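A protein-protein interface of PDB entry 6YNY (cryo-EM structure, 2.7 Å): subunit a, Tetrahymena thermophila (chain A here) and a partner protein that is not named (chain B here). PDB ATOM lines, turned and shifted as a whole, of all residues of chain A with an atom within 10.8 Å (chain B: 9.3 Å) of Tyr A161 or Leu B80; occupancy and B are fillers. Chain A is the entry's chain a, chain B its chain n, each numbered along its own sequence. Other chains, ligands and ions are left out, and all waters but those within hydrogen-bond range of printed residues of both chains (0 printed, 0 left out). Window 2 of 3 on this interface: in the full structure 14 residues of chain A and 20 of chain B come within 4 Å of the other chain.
O of Lys B81 lies close to OE1 of Gln B73. The side-chain amide oxygen (OD1) of Asn B79 is in hydrogen-bond range of the backbone NH (N) of Tyr B74, at 2.8 Å. The side-chain amide oxygen (OE1) of Gln B154 lies within hydrogen-bond range of the side-chain hydroxyl (OH) of Tyr B74, at 2.8 Å.
Phe A109 touches Ala B150. Gln B154 touches Phe A159 (CG to CZ, 3.5 Å). Tyr A161 touches Tyr B74 (OH to CE2, 3.7 Å). CB of Leu B80 touches CE2 of Tyr A161, at 3.8 Å. CE1 of Tyr A161 touches CD of Lys B81, at 3.5 Å.
Of the printed residues of chain B, Phe A109 touches Ala B150. Printed residues of chain B within 4 Å of Phe A159: Gln B154. Val A160 touches none of the printed residues of chain B. Printed residues of chain B within 4 Å of Tyr A161: Tyr B74, Leu B80 and Lys B81. Asn A166 touches none of the printed residues of chain B. Printed residues of chain A within 4 Å of Tyr B74: Tyr A161. No residue of chain A comes within 4 Å of Asn B79. Of chain A, only Tyr A161 comes within 4 Å of Leu B80. Of chain A, only Tyr A161 comes within 4 Å of Lys B81. Printed residues of chain A within 4 Å of Ala B150: Phe A109 (3.6 Å). Printed residues of chain A within 4 Å of Gln B154: Phe A159. The nearest residue of chain B that does not touch Tyr A161 is Tyr B151 (4.1 Å). The nearest printed residue of chain B that does not touch Phe A109 is Gln B154 (5.4 Å).
Printed residues of chain B that touch a printed residue of chain A: Tyr B74, Leu B80, Lys B81, Ala B150 and Gln B154. Hydrophobic or aromatic side chains of chain B that line the printed part of chain A: Tyr B74, Leu B80 and Ala B150. Printed residues of chain A that touch a printed residue of chain B: Phe A109, Phe A159 and Tyr A161. Hydrophobic or aromatic side chains of chain A within 4 Å of the printed part of chain B: Phe A109, Phe A159 and Tyr A161. Along chain A the printed residues that touch a printed residue of chain B span positions 109 to 161. Among the printed residues, no Asp or Glu carboxylate lies within 4 Å of a Lys or Arg side-chain nitrogen of the other chain.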
ATOM      1  N   LEU A 108      -0.460 -23.878   3.130  1.00  0.00           N
ATOM      2  CA  LEU A 108       0.635 -24.593   3.772  1.00  0.00           C
ATOM      3  C   LEU A 108       0.664 -24.338   5.270  1.00  0.00           C
ATOM      4  O   LEU A 108       1.109 -25.196   6.041  1.00  0.00           O
ATOM      5  CB  LEU A 108       1.966 -24.170   3.161  1.00  0.00           C
ATOM      6  CG  LEU A 108       2.158 -24.358   1.664  1.00  0.00           C
ATOM      7  CD1 LEU A 108       3.511 -23.811   1.285  1.00  0.00           C
ATOM      8  CD2 LEU A 108       2.031 -25.814   1.274  1.00  0.00           C
ATOM      9  N   PHE A 109       0.202 -23.166   5.695  1.00  0.00           N
ATOM     10  CA  PHE A 109       0.176 -22.822   7.106  1.00  0.00           C
ATOM     11  C   PHE A 109      -0.816 -23.669   7.894  1.00  0.00           C
ATOM     12  O   PHE A 109      -0.705 -23.743   9.122  1.00  0.00           O
ATOM     13  CB  PHE A 109      -0.138 -21.333   7.235  1.00  0.00           C
ATOM     14  CG  PHE A 109      -0.571 -20.909   8.596  1.00  0.00           C
ATOM     15  CD1 PHE A 109       0.326 -20.862   9.639  1.00  0.00           C
ATOM     16  CD2 PHE A 109      -1.875 -20.524   8.823  1.00  0.00           C
ATOM     17  CE1 PHE A 109      -0.076 -20.460  10.893  1.00  0.00           C
ATOM     18  CE2 PHE A 109      -2.281 -20.123  10.067  1.00  0.00           C
ATOM     19  CZ  PHE A 109      -1.382 -20.086  11.106  1.00  0.00           C
ATOM     20  N   ASN A 111      -1.687 -27.172   8.574  1.00  0.00           N
ATOM     21  CA  ASN A 111      -1.342 -28.591   8.528  1.00  0.00           C
ATOM     22  C   ASN A 111      -2.224 -29.375   9.502  1.00  0.00           C
ATOM     23  O   ASN A 111      -1.780 -29.876  10.533  1.00  0.00           O
ATOM     24  CB  ASN A 111       0.137 -28.784   8.827  1.00  0.00           C
ATOM     25  CG  ASN A 111       0.634 -30.152   8.434  1.00  0.00           C
ATOM     26  OD1 ASN A 111       0.624 -31.087   9.233  1.00  0.00           O
ATOM     27  ND2 ASN A 111       1.072 -30.278   7.190  1.00  0.00           N
ATOM     28  N   GLU A 158      -3.878 -24.948  17.079  1.00  0.00           N
ATOM     29  CA  GLU A 158      -2.670 -24.794  17.874  1.00  0.00           C
ATOM     30  C   GLU A 158      -1.466 -24.580  16.969  1.00  0.00           C
ATOM     31  O   GLU A 158      -1.323 -25.245  15.939  1.00  0.00           O
ATOM     32  CB  GLU A 158      -2.443 -26.025  18.754  1.00  0.00           C
ATOM     33  CG  GLU A 158      -3.592 -26.329  19.694  1.00  0.00           C
ATOM     34  CD  GLU A 158      -3.386 -27.607  20.482  1.00  0.00           C
ATOM     35  OE1 GLU A 158      -2.503 -28.405  20.105  1.00  0.00           O
ATOM     36  OE2 GLU A 158      -4.108 -27.815  21.481  1.00  0.00           O
ATOM     37  N   PHE A 159      -0.603 -23.651  17.364  1.00  0.00           N
ATOM     38  CA  PHE A 159       0.607 -23.354  16.612  1.00  0.00           C
ATOM     39  C   PHE A 159       1.712 -24.323  17.008  1.00  0.00           C
ATOM     40  O   PHE A 159       2.058 -24.431  18.188  1.00  0.00           O
ATOM     41  CB  PHE A 159       1.050 -21.917  16.854  1.00  0.00           C
ATOM     42  CG  PHE A 159       0.222 -20.903  16.141  1.00  0.00           C
ATOM     43  CD1 PHE A 159       0.537 -20.521  14.854  1.00  0.00           C
ATOM     44  CD2 PHE A 159      -0.867 -20.323  16.756  1.00  0.00           C
ATOM     45  CE1 PHE A 159      -0.217 -19.589  14.197  1.00  0.00           C
ATOM     46  CE2 PHE A 159      -1.623 -19.389  16.098  1.00  0.00           C
ATOM     47  CZ  PHE A 159      -1.297 -19.022  14.817  1.00  0.00           C
ATOM     48  N   VAL A 160       2.257 -25.029  16.022  1.00  0.00           N
ATOM     49  CA  VAL A 160       3.387 -25.921  16.222  1.00  0.00           C
ATOM     50  C   VAL A 160       4.392 -25.673  15.109  1.00  0.00           C
ATOM     51  O   VAL A 160       4.075 -25.089  14.072  1.00  0.00           O
ATOM     52  CB  VAL A 160       2.970 -27.405  16.244  1.00  0.00           C
ATOM     53  CG1 VAL A 160       1.915 -27.645  17.292  1.00  0.00           C
ATOM     54  CG2 VAL A 160       2.475 -27.832  14.888  1.00  0.00           C
ATOM     55  N   TYR A 161       5.619 -26.127  15.338  1.00  0.00           N
ATOM     56  CA  TYR A 161       6.672 -26.033  14.340  1.00  0.00           C
ATOM     57  C   TYR A 161       6.687 -27.322  13.528  1.00  0.00           C
ATOM     58  O   TYR A 161       6.828 -28.415  14.085  1.00  0.00           O
ATOM     59  CB  TYR A 161       8.025 -25.769  14.995  1.00  0.00           C
ATOM     60  CG  TYR A 161       8.108 -24.437  15.701  1.00  0.00           C
ATOM     61  CD1 TYR A 161       7.993 -23.252  14.997  1.00  0.00           C
ATOM     62  CD2 TYR A 161       8.305 -24.365  17.068  1.00  0.00           C
ATOM     63  CE1 TYR A 161       8.065 -22.041  15.634  1.00  0.00           C
ATOM     64  CE2 TYR A 161       8.378 -23.155  17.709  1.00  0.00           C
ATOM     65  CZ  TYR A 161       8.260 -21.996  16.989  1.00  0.00           C
ATOM     66  OH  TYR A 161       8.334 -20.783  17.630  1.00  0.00           O
ATOM     67  N   PHE A 162       6.527 -27.186  12.217  1.00  0.00           N
ATOM     68  CA  PHE A 162       6.379 -28.318  11.311  1.00  0.00           C
ATOM     69  C   PHE A 162       7.755 -28.740  10.811  1.00  0.00           C
ATOM     70  O   PHE A 162       8.406 -28.003  10.065  1.00  0.00           O
ATOM     71  CB  PHE A 162       5.456 -27.931  10.161  1.00  0.00           C
ATOM     72  CG  PHE A 162       5.211 -29.021   9.172  1.00  0.00           C
ATOM     73  CD1 PHE A 162       5.792 -28.975   7.924  1.00  0.00           C
ATOM     74  CD2 PHE A 162       4.385 -30.080   9.477  1.00  0.00           C
ATOM     75  CE1 PHE A 162       5.562 -29.967   7.005  1.00  0.00           C
ATOM     76  CE2 PHE A 162       4.152 -31.074   8.561  1.00  0.00           C
ATOM     77  CZ  PHE A 162       4.741 -31.017   7.325  1.00  0.00           C
ATOM     78  N   ASP A 163       8.195 -29.923  11.222  1.00  0.00           N
ATOM     79  CA  ASP A 163       9.517 -30.420  10.868  1.00  0.00           C
ATOM     80  C   ASP A 163       9.519 -30.899   9.422  1.00  0.00           C
ATOM     81  O   ASP A 163       8.804 -31.843   9.072  1.00  0.00           O
ATOM     82  CB  ASP A 163       9.923 -31.546  11.812  1.00  0.00           C
ATOM     83  CG  ASP A 163      11.376 -31.934  11.671  1.00  0.00           C
ATOM     84  OD1 ASP A 163      12.060 -31.385  10.783  1.00  0.00           O
ATOM     85  OD2 ASP A 163      11.839 -32.789  12.454  1.00  0.00           O
ATOM     86  N   LYS A 164      10.320 -30.244   8.583  1.00  0.00           N
ATOM     87  CA  LYS A 164      10.462 -30.660   7.195  1.00  0.00           C
ATOM     88  C   LYS A 164      11.342 -31.889   7.054  1.00  0.00           C
ATOM     89  O   LYS A 164      11.220 -32.614   6.062  1.00  0.00           O
ATOM     90  CB  LYS A 164      11.040 -29.521   6.357  1.00  0.00           C
ATOM     91  CG  LYS A 164      10.157 -28.299   6.248  1.00  0.00           C
ATOM     92  CD  LYS A 164       8.867 -28.614   5.539  1.00  0.00           C
ATOM     93  CE  LYS A 164       8.114 -27.353   5.174  1.00  0.00           C
ATOM     94  NZ  LYS A 164       8.842 -26.555   4.156  1.00  0.00           N
ATOM     95  N   SER A 165      12.226 -32.130   8.014  1.00  0.00           N
ATOM     96  CA  SER A 165      13.058 -33.323   8.018  1.00  0.00           C
ATOM     97  C   SER A 165      12.224 -34.508   8.479  1.00  0.00           C
ATOM     98  O   SER A 165      11.644 -34.484   9.569  1.00  0.00           O
ATOM     99  CB  SER A 165      14.264 -33.124   8.927  1.00  0.00           C
ATOM    100  OG  SER A 165      13.859 -32.783  10.236  1.00  0.00           O
ATOM    101  N   ASN A 166      12.160 -35.543   7.646  1.00  0.00           N
ATOM    102  CA  ASN A 166      11.347 -36.723   7.911  1.00  0.00           C
ATOM    103  C   ASN A 166      12.263 -37.905   8.186  1.00  0.00           C
ATOM    104  O   ASN A 166      12.633 -38.640   7.261  1.00  0.00           O
ATOM    105  CB  ASN A 166      10.418 -37.013   6.734  1.00  0.00           C
ATOM    106  CG  ASN A 166       9.259 -36.055   6.661  1.00  0.00           C
ATOM    107  OD1 ASN A 166       8.140 -36.385   7.047  1.00  0.00           O
ATOM    108  ND2 ASN A 166       9.518 -34.856   6.172  1.00  0.00           N
ATOM    109  N   TYR B  72       7.750  -9.908  18.140  1.00  0.00           N
ATOM    110  CA  TYR B  72       7.415 -11.179  17.512  1.00  0.00           C
ATOM    111  C   TYR B  72       7.890 -12.362  18.345  1.00  0.00           C
ATOM    112  O   TYR B  72       8.040 -13.470  17.823  1.00  0.00           O
ATOM    113  CB  TYR B  72       7.989 -11.235  16.096  1.00  0.00           C
ATOM    114  CG  TYR B  72       7.321 -10.249  15.171  1.00  0.00           C
ATOM    115  CD1 TYR B  72       7.799  -8.956  15.041  1.00  0.00           C
ATOM    116  CD2 TYR B  72       6.198 -10.606  14.448  1.00  0.00           C
ATOM    117  CE1 TYR B  72       7.182  -8.054  14.208  1.00  0.00           C
ATOM    118  CE2 TYR B  72       5.577  -9.709  13.612  1.00  0.00           C
ATOM    119  CZ  TYR B  72       6.072  -8.436  13.497  1.00  0.00           C
ATOM    120  OH  TYR B  72       5.451  -7.541  12.664  1.00  0.00           O
ATOM    121  N   GLN B  73       8.132 -12.142  19.632  1.00  0.00           N
ATOM    122  CA  GLN B  73       8.442 -13.204  20.573  1.00  0.00           C
ATOM    123  C   GLN B  73       7.231 -13.475  21.455  1.00  0.00           C
ATOM    124  O   GLN B  73       6.449 -12.572  21.763  1.00  0.00           O
ATOM    125  CB  GLN B  73       9.648 -12.834  21.436  1.00  0.00           C
ATOM    126  CG  GLN B  73      10.933 -12.654  20.659  1.00  0.00           C
ATOM    127  CD  GLN B  73      11.326 -13.889  19.882  1.00  0.00           C
ATOM    128  OE1 GLN B  73      10.995 -14.030  18.707  1.00  0.00           O
ATOM    129  NE2 GLN B  73      12.045 -14.786  20.532  1.00  0.00           N
ATOM    130  N   TYR B  74       7.080 -14.732  21.853  1.00  0.00           N
ATOM    131  CA  TYR B  74       5.943 -15.141  22.661  1.00  0.00           C
ATOM    132  C   TYR B  74       6.177 -14.808  24.126  1.00  0.00           C
ATOM    133  O   TYR B  74       7.296 -14.916  24.633  1.00  0.00           O
ATOM    134  CB  TYR B  74       5.689 -16.638  22.502  1.00  0.00           C
ATOM    135  CG  TYR B  74       5.458 -17.083  21.084  1.00  0.00           C
ATOM    136  CD1 TYR B  74       4.714 -16.317  20.205  1.00  0.00           C
ATOM    137  CD2 TYR B  74       5.990 -18.273  20.620  1.00  0.00           C
ATOM    138  CE1 TYR B  74       4.507 -16.724  18.912  1.00  0.00           C
ATOM    139  CE2 TYR B  74       5.786 -18.686  19.332  1.00  0.00           C
ATOM    140  CZ  TYR B  74       5.045 -17.911  18.480  1.00  0.00           C
ATOM    141  OH  TYR B  74       4.844 -18.329  17.189  1.00  0.00           O
ATOM    142  N   LYS B  77       4.691 -18.494  25.997  1.00  0.00           N
ATOM    143  CA  LYS B  77       5.115 -19.715  25.334  1.00  0.00           C
ATOM    144  C   LYS B  77       6.619 -19.675  25.124  1.00  0.00           C
ATOM    145  O   LYS B  77       7.213 -18.606  24.972  1.00  0.00           O
ATOM    146  CB  LYS B  77       4.409 -19.906  23.991  1.00  0.00           C
ATOM    147  CG  LYS B  77       2.960 -20.299  24.105  1.00  0.00           C
ATOM    148  CD  LYS B  77       2.170 -19.858  22.894  1.00  0.00           C
ATOM    149  CE  LYS B  77       2.755 -20.400  21.619  1.00  0.00           C
ATOM    150  NZ  LYS B  77       2.033 -19.879  20.438  1.00  0.00           N
ATOM    151  N   ALA B  78       7.226 -20.856  25.122  1.00  0.00           N
ATOM    152  CA  ALA B  78       8.658 -20.954  24.903  1.00  0.00           C
ATOM    153  C   ALA B  78       9.035 -20.389  23.541  1.00  0.00           C
ATOM    154  O   ALA B  78       8.345 -20.608  22.543  1.00  0.00           O
ATOM    155  CB  ALA B  78       9.107 -22.406  25.009  1.00  0.00           C
ATOM    156  N   ASN B  79      10.140 -19.658  23.508  1.00  0.00           N
ATOM    157  CA  ASN B  79      10.627 -19.021  22.291  1.00  0.00           C
ATOM    158  C   ASN B  79      11.692 -19.920  21.682  1.00  0.00           C
ATOM    159  O   ASN B  79      12.834 -19.955  22.142  1.00  0.00           O
ATOM    160  CB  ASN B  79      11.159 -17.627  22.587  1.00  0.00           C
ATOM    161  CG  ASN B  79      10.055 -16.630  22.815  1.00  0.00           C
ATOM    162  OD1 ASN B  79       9.582 -15.988  21.882  1.00  0.00           O
ATOM    163  ND2 ASN B  79       9.627 -16.504  24.056  1.00  0.00           N
ATOM    164  N   LEU B  80      11.303 -20.647  20.640  1.00  0.00           N
ATOM    165  CA  LEU B  80      12.189 -21.547  19.926  1.00  0.00           C
ATOM    166  C   LEU B  80      12.598 -21.002  18.568  1.00  0.00           C
ATOM    167  O   LEU B  80      13.392 -21.640  17.872  1.00  0.00           O
ATOM    168  CB  LEU B  80      11.515 -22.909  19.761  1.00  0.00           C
ATOM    169  CG  LEU B  80      10.960 -23.499  21.053  1.00  0.00           C
ATOM    170  CD1 LEU B  80      10.209 -24.776  20.788  1.00  0.00           C
ATOM    171  CD2 LEU B  80      12.069 -23.733  22.044  1.00  0.00           C
ATOM    172  N   LYS B  81      12.072 -19.847  18.176  1.00  0.00           N
ATOM    173  CA  LYS B  81      12.419 -19.223  16.911  1.00  0.00           C
ATOM    174  C   LYS B  81      12.408 -17.714  17.066  1.00  0.00           C
ATOM    175  O   LYS B  81      11.690 -17.163  17.904  1.00  0.00           O
ATOM    176  CB  LYS B  81      11.455 -19.612  15.789  1.00  0.00           C
ATOM    177  CG  LYS B  81      11.688 -20.970  15.200  1.00  0.00           C
ATOM    178  CD  LYS B  81      10.967 -21.098  13.882  1.00  0.00           C
ATOM    179  CE  LYS B  81      11.067 -22.495  13.317  1.00  0.00           C
ATOM    180  NZ  LYS B  81      12.468 -22.940  13.169  1.00  0.00           N
ATOM    181  N   THR B  82      13.218 -17.056  16.249  1.00  0.00           N
ATOM    182  CA  THR B  82      13.193 -15.615  16.095  1.00  0.00           C
ATOM    183  C   THR B  82      12.800 -15.277  14.665  1.00  0.00           C
ATOM    184  O   THR B  82      12.747 -16.141  13.786  1.00  0.00           O
ATOM    185  CB  THR B  82      14.550 -14.988  16.425  1.00  0.00           C
ATOM    186  OG1 THR B  82      15.573 -15.610  15.639  1.00  0.00           O
ATOM    187  CG2 THR B  82      14.869 -15.145  17.885  1.00  0.00           C
ATOM    188  N   LEU B  83      12.516 -14.006  14.445  1.00  0.00           N
ATOM    189  CA  LEU B  83      12.240 -13.496  13.112  1.00  0.00           C
ATOM    190  C   LEU B  83      13.370 -12.547  12.737  1.00  0.00           C
ATOM    191  O   LEU B  83      13.213 -11.324  12.828  1.00  0.00           O
ATOM    192  CB  LEU B  83      10.885 -12.799  13.070  1.00  0.00           C
ATOM    193  CG  LEU B  83      10.279 -12.567  11.690  1.00  0.00           C
ATOM    194  CD1 LEU B  83       9.869 -13.880  11.052  1.00  0.00           C
ATOM    195  CD2 LEU B  83       9.097 -11.650  11.817  1.00  0.00           C
ATOM    196  N   LEU B 147       7.416 -18.362   7.012  1.00  0.00           N
ATOM    197  CA  LEU B 147       7.369 -17.955   8.410  1.00  0.00           C
ATOM    198  C   LEU B 147       6.666 -16.616   8.566  1.00  0.00           C
ATOM    199  O   LEU B 147       5.822 -16.444   9.452  1.00  0.00           O
ATOM    200  CB  LEU B 147       8.783 -17.878   8.977  1.00  0.00           C
ATOM    201  CG  LEU B 147       9.536 -19.191   9.142  1.00  0.00           C
ATOM    202  CD1 LEU B 147      10.983 -18.904   9.436  1.00  0.00           C
ATOM    203  CD2 LEU B 147       8.924 -20.016  10.250  1.00  0.00           C
ATOM    204  N   ALA B 150       3.062 -16.932   8.429  1.00  0.00           N
ATOM    205  CA  ALA B 150       2.513 -17.524   9.642  1.00  0.00           C
ATOM    206  C   ALA B 150       2.560 -16.547  10.807  1.00  0.00           C
ATOM    207  O   ALA B 150       1.592 -16.432  11.565  1.00  0.00           O
ATOM    208  CB  ALA B 150       3.270 -18.802   9.981  1.00  0.00           C
ATOM    209  N   TYR B 151       3.676 -15.839  10.973  1.00  0.00           N
ATOM    210  CA  TYR B 151       3.748 -14.828  12.019  1.00  0.00           C
ATOM    211  C   TYR B 151       2.781 -13.684  11.756  1.00  0.00           C
ATOM    212  O   TYR B 151       2.223 -13.118  12.700  1.00  0.00           O
ATOM    213  CB  TYR B 151       5.172 -14.294  12.139  1.00  0.00           C
ATOM    214  CG  TYR B 151       6.075 -15.128  13.010  1.00  0.00           C
ATOM    215  CD1 TYR B 151       5.976 -15.073  14.389  1.00  0.00           C
ATOM    216  CD2 TYR B 151       7.037 -15.954  12.457  1.00  0.00           C
ATOM    217  CE1 TYR B 151       6.798 -15.821  15.189  1.00  0.00           C
ATOM    218  CE2 TYR B 151       7.867 -16.709  13.253  1.00  0.00           C
ATOM    219  CZ  TYR B 151       7.743 -16.637  14.619  1.00  0.00           C
ATOM    220  OH  TYR B 151       8.568 -17.388  15.419  1.00  0.00           O
ATOM    221  N   GLN B 154      -0.625 -14.985  12.737  1.00  0.00           N
ATOM    222  CA  GLN B 154      -0.650 -15.072  14.190  1.00  0.00           C
ATOM    223  C   GLN B 154      -0.677 -13.689  14.826  1.00  0.00           C
ATOM    224  O   GLN B 154      -1.214 -13.519  15.924  1.00  0.00           O
ATOM    225  CB  GLN B 154       0.559 -15.869  14.673  1.00  0.00           C
ATOM    226  CG  GLN B 154       0.515 -16.268  16.124  1.00  0.00           C
ATOM    227  CD  GLN B 154       1.665 -17.165  16.505  1.00  0.00           C
ATOM    228  OE1 GLN B 154       2.616 -17.332  15.746  1.00  0.00           O
ATOM    229  NE2 GLN B 154       1.579 -17.757  17.683  1.00  0.00           N
ATOM    230  N   PHE B 162       1.965 -12.414  21.783  1.00  0.00           N
ATOM    231  CA  PHE B 162       3.273 -11.800  21.629  1.00  0.00           C
ATOM    232  C   PHE B 162       3.577 -10.812  22.748  1.00  0.00           C
ATOM    233  O   PHE B 162       2.684 -10.262  23.395  1.00  0.00           O
ATOM    234  CB  PHE B 162       3.366 -11.088  20.281  1.00  0.00           C
ATOM    235  CG  PHE B 162       3.193 -11.996  19.111  1.00  0.00           C
ATOM    236  CD1 PHE B 162       4.272 -12.660  18.570  1.00  0.00           C
ATOM    237  CD2 PHE B 162       1.950 -12.190  18.553  1.00  0.00           C
ATOM    238  CE1 PHE B 162       4.112 -13.498  17.497  1.00  0.00           C
ATOM    239  CE2 PHE B 162       1.786 -13.024  17.482  1.00  0.00           C
ATOM    240  CZ  PHE B 162       2.866 -13.679  16.952  1.00  0.00           C
